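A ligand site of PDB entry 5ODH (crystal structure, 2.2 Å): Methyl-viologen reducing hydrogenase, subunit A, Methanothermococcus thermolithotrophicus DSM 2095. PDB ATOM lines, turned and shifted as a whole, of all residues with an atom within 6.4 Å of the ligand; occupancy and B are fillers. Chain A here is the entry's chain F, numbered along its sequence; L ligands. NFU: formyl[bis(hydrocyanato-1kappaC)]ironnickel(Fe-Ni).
An iron atom (FE) of the ligand is bound by the side-chain sulfur (SG) of Cys 445 (2.7 Å).
A nickel atom (NI) of the ligand is bound by the side-chain sulfur of Cys 64.
SG of Cys 442 binds NI of the ligand, at 2.7 Å.
A nitrogen (N2) of the ligand lies close to the backbone NH (N) of Thr 399 (3.3 Å).
OG1 of Thr 399 sits at hydrogen-bond distance from N2 of the ligand, at 2.8 Å.
NI of the ligand is bound by SG of Cys 61, at 2.8 Å.
The backbone NH of Arg 375 lies within hydrogen-bond range of a nitrogen (N1) of the ligand, 3.1 Å away.
The guanidinium group (NH1) of Arg 375 is in hydrogen-bond range of a nitrogen (N1) of the ligand (3.1 Å).
The side-chain sulfur (SG) of Cys 445 sits close to a ring nitrogen (NE2) of His 68, 2.8 Å away.
N of Cys 442 sits at hydrogen-bond distance from OG1 of Thr 399.
The side-chain sulfur (SG) of Cys 442 sits close to the side-chain carboxylate (OE1) of Glu 13 (3.0 Å).
The backbone NH (N) of Ile 63 lies close to the side-chain sulfur (SG) of Cys 61, at 3.1 Å.
NH1 of Arg 375 is in hydrogen-bond range of OG of Ser 103 (2.6 Å).
N of Leu 378 is in hydrogen-bond range of O of Val 371 (2.9 Å).
A ring nitrogen (ND1) of His 68 sits at hydrogen-bond distance from a ring nitrogen (NE2) of His 380 (3.0 Å).
The backbone carbonyl oxygen (O) of Thr 377 sits at hydrogen-bond distance from the backbone NH (N) of Ala 398 (2.9 Å).
The backbone nitrogen (N) of Pro 374 lies close to a nitrogen (N1) of the ligand, 3.4 Å away.
His 68 touches the ligand.
Ala 373 touches the ligand (CB to O3, 3.1 Å).
CD1 of Leu 378 touches O3 of the ligand, at 3.1 Å.
Val 397 touches the ligand (CG1 to C3, 3.7 Å).
Ala 398 touches the ligand.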
ATOM      1  N   GLU A  13      16.321 -23.296   8.331  1.00  0.00           N
ATOM      2  CA  GLU A  13      16.093 -23.725   9.696  1.00  0.00           C
ATOM      3  C   GLU A  13      16.574 -25.166   9.842  1.00  0.00           C
ATOM      4  O   GLU A  13      16.206 -26.035   9.040  1.00  0.00           O
ATOM      5  CB  GLU A  13      14.615 -23.589  10.064  1.00  0.00           C
ATOM      6  CG  GLU A  13      14.322 -23.714  11.553  1.00  0.00           C
ATOM      7  CD  GLU A  13      14.598 -25.115  12.069  1.00  0.00           C
ATOM      8  OE1 GLU A  13      14.325 -26.077  11.314  1.00  0.00           O
ATOM      9  OE2 GLU A  13      15.106 -25.239  13.198  1.00  0.00           O
ATOM     10  N   ILE A  60       8.611 -28.298  18.487  1.00  0.00           N
ATOM     11  CA  ILE A  60       9.208 -28.883  17.295  1.00  0.00           C
ATOM     12  C   ILE A  60       9.920 -27.817  16.486  1.00  0.00           C
ATOM     13  O   ILE A  60      10.967 -28.075  15.885  1.00  0.00           O
ATOM     14  CB  ILE A  60       8.137 -29.599  16.460  1.00  0.00           C
ATOM     15  CG1 ILE A  60       7.572 -30.798  17.222  1.00  0.00           C
ATOM     16  CG2 ILE A  60       8.723 -30.041  15.127  1.00  0.00           C
ATOM     17  CD1 ILE A  60       6.411 -31.492  16.528  1.00  0.00           C
ATOM     18  N   CYS A  61       9.371 -26.604  16.466  1.00  0.00           N
ATOM     19  CA  CYS A  61       9.968 -25.527  15.701  1.00  0.00           C
ATOM     20  C   CYS A  61       9.492 -24.181  16.207  1.00  0.00           C
ATOM     21  O   CYS A  61       8.321 -24.005  16.540  1.00  0.00           O
ATOM     22  CB  CYS A  61       9.634 -25.649  14.215  1.00  0.00           C
ATOM     23  SG  CYS A  61      10.247 -24.245  13.303  1.00  0.00           S
ATOM     24  N   GLY A  62      10.399 -23.203  16.196  1.00  0.00           N
ATOM     25  CA  GLY A  62      10.067 -21.861  16.612  1.00  0.00           C
ATOM     26  C   GLY A  62       9.498 -20.962  15.552  1.00  0.00           C
ATOM     27  O   GLY A  62       8.932 -19.907  15.884  1.00  0.00           O
ATOM     28  N   ILE A  63       9.607 -21.340  14.270  1.00  0.00           N
ATOM     29  CA  ILE A  63       9.029 -20.552  13.196  1.00  0.00           C
ATOM     30  C   ILE A  63       7.549 -20.869  13.034  1.00  0.00           C
ATOM     31  O   ILE A  63       6.702 -19.965  13.014  1.00  0.00           O
ATOM     32  CB  ILE A  63       9.800 -20.785  11.885  1.00  0.00           C
ATOM     33  CG1 ILE A  63      11.255 -20.334  12.034  1.00  0.00           C
ATOM     34  CG2 ILE A  63       9.119 -20.061  10.730  1.00  0.00           C
ATOM     35  CD1 ILE A  63      12.114 -20.623  10.803  1.00  0.00           C
ATOM     36  N   CYS A  64       7.223 -22.150  12.920  1.00  0.00           N
ATOM     37  CA  CYS A  64       5.857 -22.593  12.649  1.00  0.00           C
ATOM     38  C   CYS A  64       5.174 -23.148  13.883  1.00  0.00           C
ATOM     39  O   CYS A  64       4.245 -23.966  13.759  1.00  0.00           O
ATOM     40  CB  CYS A  64       5.859 -23.651  11.556  1.00  0.00           C
ATOM     41  SG  CYS A  64       6.380 -25.237  12.232  1.00  0.00           S
ATOM     42  N   GLN A  65       5.607 -22.745  15.074  1.00  0.00           N
ATOM     43  CA  GLN A  65       5.035 -23.287  16.305  1.00  0.00           C
ATOM     44  C   GLN A  65       3.519 -23.101  16.325  1.00  0.00           C
ATOM     45  O   GLN A  65       2.807 -23.875  16.969  1.00  0.00           O
ATOM     46  CB  GLN A  65       5.670 -22.656  17.552  1.00  0.00           C
ATOM     47  CG  GLN A  65       6.506 -21.380  17.346  1.00  0.00           C
ATOM     48  CD  GLN A  65       5.646 -20.165  17.089  1.00  0.00           C
ATOM     49  OE1 GLN A  65       4.479 -20.118  17.478  1.00  0.00           O
ATOM     50  NE2 GLN A  65       6.231 -19.161  16.450  1.00  0.00           N
ATOM     51  N   ALA A  67       1.487 -23.474  13.712  1.00  0.00           N
ATOM     52  CA  ALA A  67       0.889 -24.564  12.949  1.00  0.00           C
ATOM     53  C   ALA A  67       0.795 -25.826  13.788  1.00  0.00           C
ATOM     54  O   ALA A  67      -0.227 -26.525  13.765  1.00  0.00           O
ATOM     55  CB  ALA A  67       1.692 -24.808  11.671  1.00  0.00           C
ATOM     56  N   HIS A  68       1.855 -26.145  14.539  1.00  0.00           N
ATOM     57  CA  HIS A  68       1.819 -27.333  15.390  1.00  0.00           C
ATOM     58  C   HIS A  68       0.807 -27.173  16.512  1.00  0.00           C
ATOM     59  O   HIS A  68       0.058 -28.110  16.820  1.00  0.00           O
ATOM     60  CB  HIS A  68       3.202 -27.613  15.969  1.00  0.00           C
ATOM     61  CG  HIS A  68       4.195 -28.067  14.950  1.00  0.00           C
ATOM     62  ND1 HIS A  68       4.191 -29.348  14.417  1.00  0.00           N
ATOM     63  CD2 HIS A  68       5.235 -27.427  14.371  1.00  0.00           C
ATOM     64  CE1 HIS A  68       5.181 -29.468  13.557  1.00  0.00           C
ATOM     65  NE2 HIS A  68       5.828 -28.317  13.502  1.00  0.00           N
ATOM     66  N   SER A 103       5.918 -16.175   8.806  1.00  0.00           N
ATOM     67  CA  SER A 103       6.838 -17.204   8.322  1.00  0.00           C
ATOM     68  C   SER A 103       7.292 -16.906   6.909  1.00  0.00           C
ATOM     69  O   SER A 103       8.493 -16.961   6.596  1.00  0.00           O
ATOM     70  CB  SER A 103       6.180 -18.585   8.398  1.00  0.00           C
ATOM     71  OG  SER A 103       7.069 -19.588   7.930  1.00  0.00           O
ATOM     72  N   VAL A 371      -3.511 -29.243   9.178  1.00  0.00           N
ATOM     73  CA  VAL A 371      -3.532 -27.856   8.734  1.00  0.00           C
ATOM     74  C   VAL A 371      -2.399 -27.730   7.720  1.00  0.00           C
ATOM     75  O   VAL A 371      -1.446 -28.510   7.731  1.00  0.00           O
ATOM     76  CB  VAL A 371      -3.337 -26.857   9.905  1.00  0.00           C
ATOM     77  CG1 VAL A 371      -4.257 -27.207  11.063  1.00  0.00           C
ATOM     78  CG2 VAL A 371      -1.886 -26.776  10.360  1.00  0.00           C
ATOM     79  N   ALA A 373       0.684 -26.085   7.073  1.00  0.00           N
ATOM     80  CA  ALA A 373       1.727 -25.257   7.635  1.00  0.00           C
ATOM     81  C   ALA A 373       2.353 -24.421   6.526  1.00  0.00           C
ATOM     82  O   ALA A 373       2.185 -24.722   5.334  1.00  0.00           O
ATOM     83  CB  ALA A 373       2.794 -26.125   8.302  1.00  0.00           C
ATOM     84  N   PRO A 374       3.072 -23.363   6.882  1.00  0.00           N
ATOM     85  CA  PRO A 374       3.727 -22.558   5.843  1.00  0.00           C
ATOM     86  C   PRO A 374       4.539 -23.385   4.874  1.00  0.00           C
ATOM     87  O   PRO A 374       4.676 -23.006   3.704  1.00  0.00           O
ATOM     88  CB  PRO A 374       4.608 -21.595   6.652  1.00  0.00           C
ATOM     89  CG  PRO A 374       3.880 -21.435   7.935  1.00  0.00           C
ATOM     90  CD  PRO A 374       3.226 -22.758   8.221  1.00  0.00           C
ATOM     91  N   ARG A 375       5.082 -24.516   5.324  1.00  0.00           N
ATOM     92  CA  ARG A 375       5.959 -25.331   4.498  1.00  0.00           C
ATOM     93  C   ARG A 375       5.308 -26.643   4.079  1.00  0.00           C
ATOM     94  O   ARG A 375       6.007 -27.568   3.665  1.00  0.00           O
ATOM     95  CB  ARG A 375       7.266 -25.606   5.240  1.00  0.00           C
ATOM     96  CG  ARG A 375       8.112 -24.368   5.376  1.00  0.00           C
ATOM     97  CD  ARG A 375       9.005 -24.388   6.601  1.00  0.00           C
ATOM     98  NE  ARG A 375       9.728 -23.130   6.718  1.00  0.00           N
ATOM     99  CZ  ARG A 375       9.228 -22.035   7.290  1.00  0.00           C
ATOM    100  NH1 ARG A 375       8.009 -22.048   7.808  1.00  0.00           N
ATOM    101  NH2 ARG A 375       9.947 -20.926   7.331  1.00  0.00           N
ATOM    102  N   GLY A 376       3.982 -26.741   4.191  1.00  0.00           N
ATOM    103  CA  GLY A 376       3.277 -27.848   3.587  1.00  0.00           C
ATOM    104  C   GLY A 376       2.322 -28.498   4.551  1.00  0.00           C
ATOM    105  O   GLY A 376       2.118 -28.038   5.687  1.00  0.00           O
ATOM    106  N   THR A 377       1.741 -29.599   4.100  1.00  0.00           N
ATOM    107  CA  THR A 377       0.728 -30.299   4.872  1.00  0.00           C
ATOM    108  C   THR A 377       1.329 -30.774   6.183  1.00  0.00           C
ATOM    109  O   THR A 377       2.423 -31.337   6.227  1.00  0.00           O
ATOM    110  CB  THR A 377       0.189 -31.491   4.082  1.00  0.00           C
ATOM    111  OG1 THR A 377      -0.224 -31.051   2.785  1.00  0.00           O
ATOM    112  CG2 THR A 377      -0.982 -32.131   4.807  1.00  0.00           C
ATOM    113  N   LEU A 378       0.600 -30.521   7.269  1.00  0.00           N
ATOM    114  CA  LEU A 378       1.024 -30.867   8.610  1.00  0.00           C
ATOM    115  C   LEU A 378      -0.045 -31.747   9.234  1.00  0.00           C
ATOM    116  O   LEU A 378      -1.202 -31.323   9.338  1.00  0.00           O
ATOM    117  CB  LEU A 378       1.258 -29.616   9.452  1.00  0.00           C
ATOM    118  CG  LEU A 378       1.486 -29.831  10.944  1.00  0.00           C
ATOM    119  CD1 LEU A 378       2.831 -30.489  11.185  1.00  0.00           C
ATOM    120  CD2 LEU A 378       1.374 -28.516  11.705  1.00  0.00           C
ATOM    121  N   HIS A 380      -0.993 -34.209  12.564  1.00  0.00           N
ATOM    122  CA  HIS A 380      -0.757 -34.735  13.902  1.00  0.00           C
ATOM    123  C   HIS A 380      -1.769 -35.834  14.171  1.00  0.00           C
ATOM    124  O   HIS A 380      -2.982 -35.591  14.126  1.00  0.00           O
ATOM    125  CB  HIS A 380      -0.879 -33.633  14.968  1.00  0.00           C
ATOM    126  CG  HIS A 380       0.257 -32.651  14.951  1.00  0.00           C
ATOM    127  ND1 HIS A 380       0.461 -31.747  15.971  1.00  0.00           N
ATOM    128  CD2 HIS A 380       1.231 -32.426  14.045  1.00  0.00           C
ATOM    129  CE1 HIS A 380       1.533 -31.015  15.689  1.00  0.00           C
ATOM    130  NE2 HIS A 380       2.016 -31.404  14.525  1.00  0.00           N
ATOM    131  N   VAL A 396       3.399 -36.258  10.369  1.00  0.00           N
ATOM    132  CA  VAL A 396       3.846 -36.022   9.002  1.00  0.00           C
ATOM    133  C   VAL A 396       3.987 -34.506   8.864  1.00  0.00           C
ATOM    134  O   VAL A 396       2.987 -33.796   8.718  1.00  0.00           O
ATOM    135  CB  VAL A 396       2.878 -36.608   7.966  1.00  0.00           C
ATOM    136  CG1 VAL A 396       3.412 -36.387   6.565  1.00  0.00           C
ATOM    137  CG2 VAL A 396       2.647 -38.084   8.231  1.00  0.00           C
ATOM    138  N   VAL A 397       5.225 -34.021   8.908  1.00  0.00           N
ATOM    139  CA  VAL A 397       5.482 -32.605   9.121  1.00  0.00           C
ATOM    140  C   VAL A 397       6.060 -32.019   7.845  1.00  0.00           C
ATOM    141  O   VAL A 397       7.268 -32.118   7.583  1.00  0.00           O
ATOM    142  CB  VAL A 397       6.411 -32.361  10.321  1.00  0.00           C
ATOM    143  CG1 VAL A 397       6.620 -30.874  10.534  1.00  0.00           C
ATOM    144  CG2 VAL A 397       5.837 -33.006  11.572  1.00  0.00           C
ATOM    145  N   ALA A 398       5.174 -31.420   7.042  1.00  0.00           N
ATOM    146  CA  ALA A 398       5.531 -30.492   5.972  1.00  0.00           C
ATOM    147  C   ALA A 398       6.813 -30.829   5.219  1.00  0.00           C
ATOM    148  O   ALA A 398       6.797 -31.640   4.299  1.00  0.00           O
ATOM    149  CB  ALA A 398       5.621 -29.084   6.554  1.00  0.00           C
ATOM    150  N   THR A 399       7.938 -30.199   5.607  1.00  0.00           N
ATOM    151  CA  THR A 399       9.155 -30.254   4.795  1.00  0.00           C
ATOM    152  C   THR A 399       9.637 -31.672   4.541  1.00  0.00           C
ATOM    153  O   THR A 399      10.393 -31.879   3.578  1.00  0.00           O
ATOM    154  CB  THR A 399      10.258 -29.438   5.480  1.00  0.00           C
ATOM    155  OG1 THR A 399      10.030 -28.038   5.259  1.00  0.00           O
ATOM    156  CG2 THR A 399      11.656 -29.784   4.946  1.00  0.00           C
ATOM    157  N   VAL A 400       9.279 -32.654   5.380  1.00  0.00           N
ATOM    158  CA  VAL A 400       9.695 -34.026   5.100  1.00  0.00           C
ATOM    159  C   VAL A 400       9.248 -34.434   3.704  1.00  0.00           C
ATOM    160  O   VAL A 400       9.963 -35.173   3.008  1.00  0.00           O
ATOM    161  CB  VAL A 400       9.139 -34.999   6.175  1.00  0.00           C
ATOM    162  CG1 VAL A 400       7.627 -35.035   6.150  1.00  0.00           C
ATOM    163  CG2 VAL A 400       9.708 -36.406   5.970  1.00  0.00           C
ATOM    164  N   ASP A 440      11.969 -23.585   1.164  1.00  0.00           N
ATOM    165  CA  ASP A 440      11.781 -23.067   2.516  1.00  0.00           C
ATOM    166  C   ASP A 440      11.867 -24.202   3.538  1.00  0.00           C
ATOM    167  O   ASP A 440      10.953 -24.393   4.352  1.00  0.00           O
ATOM    168  CB  ASP A 440      10.447 -22.331   2.632  1.00  0.00           C
ATOM    169  CG  ASP A 440      10.277 -21.623   3.965  1.00  0.00           C
ATOM    170  OD1 ASP A 440      11.265 -21.540   4.722  1.00  0.00           O
ATOM    171  OD2 ASP A 440       9.160 -21.140   4.233  1.00  0.00           O
ATOM    172  N   PRO A 441      12.964 -24.958   3.543  1.00  0.00           N
ATOM    173  CA  PRO A 441      13.038 -26.150   4.392  1.00  0.00           C
ATOM    174  C   PRO A 441      13.198 -25.791   5.865  1.00  0.00           C
ATOM    175  O   PRO A 441      13.970 -24.914   6.241  1.00  0.00           O
ATOM    176  CB  PRO A 441      14.264 -26.888   3.873  1.00  0.00           C
ATOM    177  CG  PRO A 441      15.134 -25.826   3.292  1.00  0.00           C
ATOM    178  CD  PRO A 441      14.219 -24.721   2.818  1.00  0.00           C
ATOM    179  N   CYS A 442      12.443 -26.502   6.687  1.00  0.00           N
ATOM    180  CA  CYS A 442      12.566 -26.456   8.138  1.00  0.00           C
ATOM    181  C   CYS A 442      12.974 -27.847   8.607  1.00  0.00           C
ATOM    182  O   CYS A 442      12.124 -28.754   8.680  1.00  0.00           O
ATOM    183  CB  CYS A 442      11.261 -26.009   8.772  1.00  0.00           C
ATOM    184  SG  CYS A 442      11.477 -25.558  10.477  1.00  0.00           S
ATOM    185  N   LEU A 443      14.241 -28.017   8.934  1.00  0.00           N
ATOM    186  CA  LEU A 443      14.787 -29.346   9.160  1.00  0.00           C
ATOM    187  C   LEU A 443      14.572 -29.859  10.579  1.00  0.00           C
ATOM    188  O   LEU A 443      14.550 -31.073  10.783  1.00  0.00           O
ATOM    189  CB  LEU A 443      16.283 -29.359   8.819  1.00  0.00           C
ATOM    190  CG  LEU A 443      16.641 -28.873   7.411  1.00  0.00           C
ATOM    191  CD1 LEU A 443      18.155 -28.725   7.267  1.00  0.00           C
ATOM    192  CD2 LEU A 443      16.097 -29.809   6.351  1.00  0.00           C
ATOM    193  N   SER A 444      14.411 -28.952  11.559  1.00  0.00           N
ATOM    194  CA  SER A 444      13.931 -29.377  12.860  1.00  0.00           C
ATOM    195  C   SER A 444      12.511 -29.900  12.769  1.00  0.00           C
ATOM    196  O   SER A 444      12.161 -30.894  13.408  1.00  0.00           O
ATOM    197  CB  SER A 444      14.003 -28.216  13.863  1.00  0.00           C
ATOM    198  OG  SER A 444      15.341 -27.809  14.109  1.00  0.00           O
ATOM    199  N   CYS A 445      11.677 -29.232  11.972  1.00  0.00           N
ATOM    200  CA  CYS A 445      10.297 -29.664  11.780  1.00  0.00           C
ATOM    201  C   CYS A 445      10.222 -30.974  10.999  1.00  0.00           C
ATOM    202  O   CYS A 445       9.436 -31.862  11.335  1.00  0.00           O
ATOM    203  CB  CYS A 445       9.523 -28.590  11.040  1.00  0.00           C
ATOM    204  SG  CYS A 445       8.178 -27.950  11.994  1.00  0.00           S
ATOM    205  N   ALA A 446      11.019 -31.089   9.935  1.00  0.00           N
ATOM    206  CA  ALA A 446      10.925 -32.254   9.062  1.00  0.00           C
ATOM    207  C   ALA A 446      11.272 -33.541   9.793  1.00  0.00           C
ATOM    208  O   ALA A 446      10.706 -34.600   9.495  1.00  0.00           O
ATOM    209  CB  ALA A 446      11.828 -32.039   7.857  1.00  0.00           C
HETATM  210 FE   NFU L   1       7.020 -26.693   9.912  1.00  0.00          FE
HETATM  211 NI   NFU L   1       8.836 -25.198  11.096  1.00  0.00          NI
HETATM  212  C1  NFU L   1       6.451 -25.252   8.922  1.00  0.00           C
HETATM  213  N1  NFU L   1       6.033 -24.360   8.304  1.00  0.00           N
HETATM  214  C2  NFU L   1       8.068 -27.319   8.543  1.00  0.00           C
HETATM  215  N2  NFU L   1       8.697 -27.782   7.683  1.00  0.00           N
HETATM  216  C3  NFU L   1       5.344 -27.362  10.249  1.00  0.00           C
HETATM  217  O3  NFU L   1       4.235 -27.805  10.412  1.00  0.00           O
